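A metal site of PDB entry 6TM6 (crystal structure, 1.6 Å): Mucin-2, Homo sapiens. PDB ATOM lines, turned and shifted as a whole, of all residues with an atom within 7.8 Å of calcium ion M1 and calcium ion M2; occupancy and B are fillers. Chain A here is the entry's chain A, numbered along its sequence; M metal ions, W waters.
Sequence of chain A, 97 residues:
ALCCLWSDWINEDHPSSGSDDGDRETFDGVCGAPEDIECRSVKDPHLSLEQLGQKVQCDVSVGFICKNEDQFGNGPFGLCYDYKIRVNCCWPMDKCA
A ring nitrogen (ND1) of His 14 is in hydrogen-bond range of the side-chain carboxylate (OD2) of Asp 82 (2.8 Å).
The backbone NH of Gly 22 sits close to the side-chain amide nitrogen of Asn 68.
O of Asp 82 sits at hydrogen-bond distance from N of Val 42.
The backbone NH (N) of His 14 lies close to the side-chain carboxylate (OD1) of Asp 23 (3.2 Å).
The backbone carbonyl oxygen of Glu 25 lies within hydrogen-bond range of the backbone NH of Phe 64 (2.9 Å).
OD2 of Asp 13 sits at hydrogen-bond distance from N of Arg 24 (2.8 Å).
N of Glu 12 sits at hydrogen-bond distance from OE1 of Glu 25.
The backbone carbonyl oxygen of Asp 23 sits at hydrogen-bond distance from the backbone NH of Cys 66 (2.8 Å).
Of the 26 residues printed, 6 come within 4 Å of calcium ion M1.
The nearest printed residue that does not touch calcium ion M1 is His 14 (4.2 Å).
Five residues have an atom within 4 Å of calcium ion M2: Asp 13, His 14, Ser 17, Asp 20 and Gly 22.
Calcium ion M1 is bound by O of Asp 13 (2.3 Å).
OD1 of Asn 11 binds calcium ion M1 (2.3 Å).
OD1 of Asp 82 binds calcium ion M1.
O of Tyr 83 is bound to calcium ion M1, at 2.4 Å.
Calcium ion M1 is bound by OE2 of Glu 25, at 2.4 Å.
Calcium ion M1 is bound by the side-chain carboxylate (OD2) of Asp 23, 2.5 Å away.
OD1 of Asp 23 binds calcium ion M1 (2.6 Å).
Calcium ion M1 has seven donor atoms within binding distance.
Calcium ion M2 is bound by O of Ser 17, O of His 14, water W1, O of Gly 22, OD1 of Asp 20 and OD1 of Asp 13.
Water W1 lies within hydrogen-bond range of the backbone carbonyl oxygen of Pro 15 (2.8 Å), the backbone NH of Gly 22 (3.0 Å) and the backbone NH of Asp 21 (3.3 Å).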
ATOM      1  N   ILE A  10      10.520  -7.200 -15.927  1.00  0.00           N
ATOM      2  CA  ILE A  10       9.102  -7.314 -16.286  1.00  0.00           C
ATOM      3  C   ILE A  10       8.592  -5.918 -16.640  1.00  0.00           C
ATOM      4  O   ILE A  10       8.765  -4.982 -15.867  1.00  0.00           O
ATOM      5  CB  ILE A  10       8.277  -7.911 -15.141  1.00  0.00           C
ATOM      6  CG1 ILE A  10       8.798  -9.310 -14.778  1.00  0.00           C
ATOM      7  CG2 ILE A  10       6.805  -7.931 -15.504  1.00  0.00           C
ATOM      8  CD1 ILE A  10       8.629  -9.663 -13.309  1.00  0.00           C
ATOM      9  N   ASN A  11       7.980  -5.784 -17.829  1.00  0.00           N
ATOM     10  CA  ASN A  11       7.468  -4.481 -18.271  1.00  0.00           C
ATOM     11  C   ASN A  11       6.268  -4.740 -19.180  1.00  0.00           C
ATOM     12  O   ASN A  11       6.356  -4.669 -20.406  1.00  0.00           O
ATOM     13  CB  ASN A  11       8.533  -3.635 -18.972  1.00  0.00           C
ATOM     14  CG  ASN A  11       8.030  -2.250 -19.315  1.00  0.00           C
ATOM     15  OD1 ASN A  11       6.989  -1.840 -18.830  1.00  0.00           O
ATOM     16  ND2 ASN A  11       8.764  -1.509 -20.145  1.00  0.00           N
ATOM     17  N   GLU A  12       5.132  -5.047 -18.559  1.00  0.00           N
ATOM     18  CA  GLU A  12       3.929  -5.447 -19.277  1.00  0.00           C
ATOM     19  C   GLU A  12       2.918  -4.323 -19.423  1.00  0.00           C
ATOM     20  O   GLU A  12       2.057  -4.395 -20.304  1.00  0.00           O
ATOM     21  CB  GLU A  12       3.260  -6.621 -18.572  1.00  0.00           C
ATOM     22  CG  GLU A  12       4.015  -7.925 -18.733  1.00  0.00           C
ATOM     23  CD  GLU A  12       4.181  -8.302 -20.198  1.00  0.00           C
ATOM     24  OE1 GLU A  12       3.153  -8.647 -20.828  1.00  0.00           O
ATOM     25  OE2 GLU A  12       5.314  -8.242 -20.723  1.00  0.00           O
ATOM     26  N   ASP A  13       3.007  -3.305 -18.583  1.00  0.00           N
ATOM     27  CA  ASP A  13       2.091  -2.164 -18.587  1.00  0.00           C
ATOM     28  C   ASP A  13       2.885  -0.930 -18.987  1.00  0.00           C
ATOM     29  O   ASP A  13       4.105  -0.931 -18.928  1.00  0.00           O
ATOM     30  CB  ASP A  13       1.462  -2.006 -17.192  1.00  0.00           C
ATOM     31  CG  ASP A  13       0.287  -1.026 -17.152  1.00  0.00           C
ATOM     32  OD1 ASP A  13      -0.243  -0.617 -18.200  1.00  0.00           O
ATOM     33  OD2 ASP A  13      -0.101  -0.691 -16.017  1.00  0.00           O
ATOM     34  N   HIS A  14       2.176   0.121 -19.403  1.00  0.00           N
ATOM     35  CA  HIS A  14       2.846   1.367 -19.768  1.00  0.00           C
ATOM     36  C   HIS A  14       1.927   2.523 -19.399  1.00  0.00           C
ATOM     37  O   HIS A  14       0.701   2.335 -19.361  1.00  0.00           O
ATOM     38  CB  HIS A  14       3.202   1.429 -21.257  1.00  0.00           C
ATOM     39  CG  HIS A  14       3.879   0.186 -21.745  1.00  0.00           C
ATOM     40  ND1 HIS A  14       5.229  -0.051 -21.569  1.00  0.00           N
ATOM     41  CD2 HIS A  14       3.393  -0.904 -22.382  1.00  0.00           C
ATOM     42  CE1 HIS A  14       5.541  -1.228 -22.083  1.00  0.00           C
ATOM     43  NE2 HIS A  14       4.450  -1.769 -22.582  1.00  0.00           N
ATOM     44  N   PRO A  15       2.474   3.710 -19.125  1.00  0.00           N
ATOM     45  CA  PRO A  15       1.641   4.786 -18.564  1.00  0.00           C
ATOM     46  C   PRO A  15       0.521   5.247 -19.462  1.00  0.00           C
ATOM     47  O   PRO A  15      -0.439   5.831 -18.953  1.00  0.00           O
ATOM     48  CB  PRO A  15       2.644   5.918 -18.316  1.00  0.00           C
ATOM     49  CG  PRO A  15       3.950   5.239 -18.198  1.00  0.00           C
ATOM     50  CD  PRO A  15       3.893   4.092 -19.157  1.00  0.00           C
ATOM     51  N   SER A  16       0.630   5.053 -20.781  1.00  0.00           N
ATOM     52  CA  SER A  16      -0.436   5.448 -21.700  1.00  0.00           C
ATOM     53  C   SER A  16      -1.065   4.249 -22.401  1.00  0.00           C
ATOM     54  O   SER A  16      -1.676   4.418 -23.461  1.00  0.00           O
ATOM     55  CB  SER A  16       0.086   6.457 -22.717  1.00  0.00           C
ATOM     56  OG  SER A  16       0.713   7.552 -22.060  1.00  0.00           O
ATOM     57  N   SER A  17      -0.916   3.049 -21.847  1.00  0.00           N
ATOM     58  CA  SER A  17      -1.520   1.833 -22.364  1.00  0.00           C
ATOM     59  C   SER A  17      -2.484   1.258 -21.338  1.00  0.00           C
ATOM     60  O   SER A  17      -2.338   1.491 -20.133  1.00  0.00           O
ATOM     61  CB  SER A  17      -0.470   0.771 -22.704  1.00  0.00           C
ATOM     62  OG  SER A  17       0.578   1.352 -23.438  1.00  0.00           O
ATOM     63  N   GLY A  18      -3.444   0.463 -21.821  1.00  0.00           N
ATOM     64  CA  GLY A  18      -4.386  -0.170 -20.924  1.00  0.00           C
ATOM     65  C   GLY A  18      -5.412   0.824 -20.379  1.00  0.00           C
ATOM     66  O   GLY A  18      -5.586   1.938 -20.870  1.00  0.00           O
ATOM     67  N   SER A  19      -6.071   0.389 -19.309  1.00  0.00           N
ATOM     68  CA  SER A  19      -7.206   1.105 -18.754  1.00  0.00           C
ATOM     69  C   SER A  19      -6.970   1.588 -17.322  1.00  0.00           C
ATOM     70  O   SER A  19      -7.922   2.068 -16.682  1.00  0.00           O
ATOM     71  CB  SER A  19      -8.448   0.222 -18.776  1.00  0.00           C
ATOM     72  OG  SER A  19      -8.174  -0.955 -18.046  1.00  0.00           O
ATOM     73  N   ASP A  20      -5.751   1.475 -16.808  1.00  0.00           N
ATOM     74  CA  ASP A  20      -5.505   1.786 -15.400  1.00  0.00           C
ATOM     75  C   ASP A  20      -4.981   3.196 -15.150  1.00  0.00           C
ATOM     76  O   ASP A  20      -4.795   3.559 -13.987  1.00  0.00           O
ATOM     77  CB  ASP A  20      -4.541   0.768 -14.795  1.00  0.00           C
ATOM     78  CG  ASP A  20      -3.205   0.660 -15.532  1.00  0.00           C
ATOM     79  OD1 ASP A  20      -3.050   1.145 -16.679  1.00  0.00           O
ATOM     80  OD2 ASP A  20      -2.298   0.057 -14.936  1.00  0.00           O
ATOM     81  N   ASP A  21      -4.763   3.999 -16.200  1.00  0.00           N
ATOM     82  CA  ASP A  21      -4.242   5.360 -16.044  1.00  0.00           C
ATOM     83  C   ASP A  21      -3.009   5.376 -15.130  1.00  0.00           C
ATOM     84  O   ASP A  21      -2.949   6.079 -14.115  1.00  0.00           O
ATOM     85  CB  ASP A  21      -5.313   6.319 -15.536  1.00  0.00           C
ATOM     86  CG  ASP A  21      -4.849   7.769 -15.570  1.00  0.00           C
ATOM     87  OD1 ASP A  21      -4.177   8.143 -16.550  1.00  0.00           O
ATOM     88  OD2 ASP A  21      -5.112   8.514 -14.596  1.00  0.00           O
ATOM     89  N   GLY A  22      -2.020   4.575 -15.503  1.00  0.00           N
ATOM     90  CA  GLY A  22      -0.819   4.470 -14.706  1.00  0.00           C
ATOM     91  C   GLY A  22       0.042   3.320 -15.198  1.00  0.00           C
ATOM     92  O   GLY A  22      -0.112   2.859 -16.329  1.00  0.00           O
ATOM     93  N   ASP A  23       0.977   2.911 -14.352  1.00  0.00           N
ATOM     94  CA  ASP A  23       1.860   1.780 -14.655  1.00  0.00           C
ATOM     95  C   ASP A  23       1.854   0.830 -13.479  1.00  0.00           C
ATOM     96  O   ASP A  23       2.258   1.211 -12.367  1.00  0.00           O
ATOM     97  CB  ASP A  23       3.288   2.243 -14.952  1.00  0.00           C
ATOM     98  CG  ASP A  23       4.112   1.190 -15.691  1.00  0.00           C
ATOM     99  OD1 ASP A  23       3.545   0.418 -16.481  1.00  0.00           O
ATOM    100  OD2 ASP A  23       5.322   1.140 -15.498  1.00  0.00           O
ATOM    101  N   ARG A  24       1.412  -0.406 -13.705  1.00  0.00           N
ATOM    102  CA  ARG A  24       1.452  -1.446 -12.689  1.00  0.00           C
ATOM    103  C   ARG A  24       2.201  -2.648 -13.230  1.00  0.00           C
ATOM    104  O   ARG A  24       1.944  -3.092 -14.353  1.00  0.00           O
ATOM    105  CB  ARG A  24       0.048  -1.834 -12.244  1.00  0.00           C
ATOM    106  CG  ARG A  24      -0.685  -0.632 -11.675  1.00  0.00           C
ATOM    107  CD  ARG A  24      -1.977  -0.959 -10.944  1.00  0.00           C
ATOM    108  NE  ARG A  24      -2.862   0.204 -10.979  1.00  0.00           N
ATOM    109  CZ  ARG A  24      -3.861   0.434 -10.128  1.00  0.00           C
ATOM    110  NH1 ARG A  24      -4.115  -0.403  -9.137  1.00  0.00           N
ATOM    111  NH2 ARG A  24      -4.592   1.527 -10.267  1.00  0.00           N
ATOM    112  N   GLU A  25       3.136  -3.154 -12.440  1.00  0.00           N
ATOM    113  CA  GLU A  25       3.875  -4.355 -12.793  1.00  0.00           C
ATOM    114  C   GLU A  25       3.733  -5.374 -11.689  1.00  0.00           C
ATOM    115  O   GLU A  25       3.851  -5.039 -10.497  1.00  0.00           O
ATOM    116  CB  GLU A  25       5.353  -4.065 -13.049  1.00  0.00           C
ATOM    117  CG  GLU A  25       5.595  -3.009 -14.139  1.00  0.00           C
ATOM    118  CD  GLU A  25       5.148  -3.454 -15.511  1.00  0.00           C
ATOM    119  OE1 GLU A  25       4.976  -4.666 -15.758  1.00  0.00           O
ATOM    120  OE2 GLU A  25       4.977  -2.572 -16.377  1.00  0.00           O
ATOM    121  N   ARG A  40      12.433   0.216 -11.524  1.00  0.00           N
ATOM    122  CA  ARG A  40      13.237   1.247 -12.181  1.00  0.00           C
ATOM    123  C   ARG A  40      12.494   1.847 -13.362  1.00  0.00           C
ATOM    124  O   ARG A  40      11.671   1.180 -14.011  1.00  0.00           O
ATOM    125  CB  ARG A  40      14.580   0.699 -12.676  1.00  0.00           C
ATOM    126  CG  ARG A  40      15.504   0.206 -11.574  1.00  0.00           C
ATOM    127  CD  ARG A  40      16.020   1.377 -10.760  1.00  0.00           C
ATOM    128  NE  ARG A  40      16.681   0.918  -9.545  1.00  0.00           N
ATOM    129  CZ  ARG A  40      17.982   0.632  -9.464  1.00  0.00           C
ATOM    130  NH1 ARG A  40      18.775   0.776 -10.523  1.00  0.00           N
ATOM    131  NH2 ARG A  40      18.489   0.195  -8.313  1.00  0.00           N
ATOM    132  N   VAL A  42      12.249   2.895 -17.148  1.00  0.00           N
ATOM    133  CA  VAL A  42      12.803   2.337 -18.384  1.00  0.00           C
ATOM    134  C   VAL A  42      13.844   3.284 -18.974  1.00  0.00           C
ATOM    135  O   VAL A  42      14.912   2.849 -19.418  1.00  0.00           O
ATOM    136  CB  VAL A  42      11.665   2.045 -19.385  1.00  0.00           C
ATOM    137  CG1 VAL A  42      12.228   1.665 -20.747  1.00  0.00           C
ATOM    138  CG2 VAL A  42      10.739   0.938 -18.844  1.00  0.00           C
ATOM    139  N   PHE A  64       4.503  -3.415  -8.204  1.00  0.00           N
ATOM    140  CA  PHE A  64       4.726  -1.999  -8.492  1.00  0.00           C
ATOM    141  C   PHE A  64       3.435  -1.319  -8.946  1.00  0.00           C
ATOM    142  O   PHE A  64       2.768  -1.822  -9.844  1.00  0.00           O
ATOM    143  CB  PHE A  64       5.793  -1.806  -9.556  1.00  0.00           C
ATOM    144  CG  PHE A  64       5.993  -0.374  -9.904  1.00  0.00           C
ATOM    145  CD1 PHE A  64       6.771   0.429  -9.093  1.00  0.00           C
ATOM    146  CD2 PHE A  64       5.349   0.201 -11.008  1.00  0.00           C
ATOM    147  CE1 PHE A  64       6.952   1.763  -9.377  1.00  0.00           C
ATOM    148  CE2 PHE A  64       5.516   1.552 -11.293  1.00  0.00           C
ATOM    149  CZ  PHE A  64       6.318   2.334 -10.473  1.00  0.00           C
ATOM    150  N   CYS A  66       2.101   2.664 -10.035  1.00  0.00           N
ATOM    151  CA  CYS A  66       2.184   4.116 -10.226  1.00  0.00           C
ATOM    152  C   CYS A  66       0.857   4.582 -10.811  1.00  0.00           C
ATOM    153  O   CYS A  66       0.369   4.006 -11.787  1.00  0.00           O
ATOM    154  CB  CYS A  66       3.341   4.496 -11.166  1.00  0.00           C
ATOM    155  SG  CYS A  66       3.558   6.300 -11.386  1.00  0.00           S
ATOM    156  N   ASN A  68      -1.121   7.776 -12.515  1.00  0.00           N
ATOM    157  CA  ASN A  68      -0.724   8.981 -13.250  1.00  0.00           C
ATOM    158  C   ASN A  68      -1.121  10.243 -12.504  1.00  0.00           C
ATOM    159  O   ASN A  68      -0.389  11.240 -12.506  1.00  0.00           O
ATOM    160  CB  ASN A  68      -1.329   8.982 -14.655  1.00  0.00           C
ATOM    161  CG  ASN A  68      -0.606   8.051 -15.623  1.00  0.00           C
ATOM    162  OD1 ASN A  68       0.565   7.754 -15.440  1.00  0.00           O
ATOM    163  ND2 ASN A  68      -1.306   7.584 -16.656  1.00  0.00           N
ATOM    164  N   TYR A  81       6.310   7.926 -15.258  1.00  0.00           N
ATOM    165  CA  TYR A  81       7.295   7.305 -16.140  1.00  0.00           C
ATOM    166  C   TYR A  81       6.863   5.863 -16.425  1.00  0.00           C
ATOM    167  O   TYR A  81       6.037   5.281 -15.719  1.00  0.00           O
ATOM    168  CB  TYR A  81       8.679   7.285 -15.501  1.00  0.00           C
ATOM    169  CG  TYR A  81       9.249   8.624 -15.134  1.00  0.00           C
ATOM    170  CD1 TYR A  81       9.106   9.730 -15.973  1.00  0.00           C
ATOM    171  CD2 TYR A  81       9.960   8.795 -13.958  1.00  0.00           C
ATOM    172  CE1 TYR A  81       9.650  10.960 -15.633  1.00  0.00           C
ATOM    173  CE2 TYR A  81      10.509  10.011 -13.616  1.00  0.00           C
ATOM    174  CZ  TYR A  81      10.342  11.094 -14.456  1.00  0.00           C
ATOM    175  OH  TYR A  81      10.880  12.313 -14.123  1.00  0.00           O
ATOM    176  N   ASP A  82       7.436   5.277 -17.484  1.00  0.00           N
ATOM    177  CA  ASP A  82       7.259   3.844 -17.670  1.00  0.00           C
ATOM    178  C   ASP A  82       8.275   3.104 -16.804  1.00  0.00           C
ATOM    179  O   ASP A  82       9.474   3.394 -16.845  1.00  0.00           O
ATOM    180  CB  ASP A  82       7.419   3.435 -19.138  1.00  0.00           C
ATOM    181  CG  ASP A  82       6.961   2.002 -19.399  1.00  0.00           C
ATOM    182  OD1 ASP A  82       6.219   1.445 -18.579  1.00  0.00           O
ATOM    183  OD2 ASP A  82       7.352   1.431 -20.431  1.00  0.00           O
ATOM    184  N   TYR A  83       7.791   2.153 -16.002  1.00  0.00           N
ATOM    185  CA  TYR A  83       8.639   1.405 -15.088  1.00  0.00           C
ATOM    186  C   TYR A  83       8.717  -0.053 -15.491  1.00  0.00           C
ATOM    187  O   TYR A  83       7.844  -0.611 -16.169  1.00  0.00           O
ATOM    188  CB  TYR A  83       8.112   1.488 -13.660  1.00  0.00           C
ATOM    189  CG  TYR A  83       8.230   2.856 -13.034  1.00  0.00           C
ATOM    190  CD1 TYR A  83       7.275   3.852 -13.294  1.00  0.00           C
ATOM    191  CD2 TYR A  83       9.271   3.146 -12.168  1.00  0.00           C
ATOM    192  CE1 TYR A  83       7.383   5.121 -12.711  1.00  0.00           C
ATOM    193  CE2 TYR A  83       9.383   4.402 -11.583  1.00  0.00           C
ATOM    194  CZ  TYR A  83       8.441   5.385 -11.865  1.00  0.00           C
ATOM    195  OH  TYR A  83       8.562   6.636 -11.281  1.00  0.00           O
ATOM    196  N   LYS A  84       9.788  -0.679 -15.020  1.00  0.00           N
ATOM    197  CA  LYS A  84      10.025  -2.113 -15.151  1.00  0.00           C
ATOM    198  C   LYS A  84      10.509  -2.620 -13.795  1.00  0.00           C
ATOM    199  O   LYS A  84      11.030  -1.853 -12.984  1.00  0.00           O
ATOM    200  CB  LYS A  84      11.040  -2.402 -16.264  1.00  0.00           C
ATOM    201  CG  LYS A  84      12.318  -1.558 -16.159  1.00  0.00           C
ATOM    202  CD  LYS A  84      13.352  -1.910 -17.224  1.00  0.00           C
ATOM    203  CE  LYS A  84      14.726  -1.342 -16.832  1.00  0.00           C
ATOM    204  NZ  LYS A  84      15.723  -1.610 -17.904  1.00  0.00           N
ATOM    205  N   ILE A  85      10.320  -3.916 -13.557  1.00  0.00           N
ATOM    206  CA  ILE A  85      10.692  -4.491 -12.269  1.00  0.00           C
ATOM    207  C   ILE A  85      11.471  -5.783 -12.469  1.00  0.00           C
ATOM    208  O   ILE A  85      11.269  -6.530 -13.436  1.00  0.00           O
ATOM    209  CB  ILE A  85       9.481  -4.755 -11.338  1.00  0.00           C
ATOM    210  CG1 ILE A  85       8.607  -5.895 -11.882  1.00  0.00           C
ATOM    211  CG2 ILE A  85       8.685  -3.481 -11.111  1.00  0.00           C
ATOM    212  CD1 ILE A  85       7.556  -6.345 -10.891  1.00  0.00           C
HETATM  213 CA    CA M   1       5.760  -0.526 -17.333  1.00  0.00          CA
HETATM  214 CA    CA M   2      -1.228   1.737 -18.164  1.00  0.00          CA
HETATM  215  O   HOH W   1      -2.294   3.870 -18.403  1.00  0.00           O
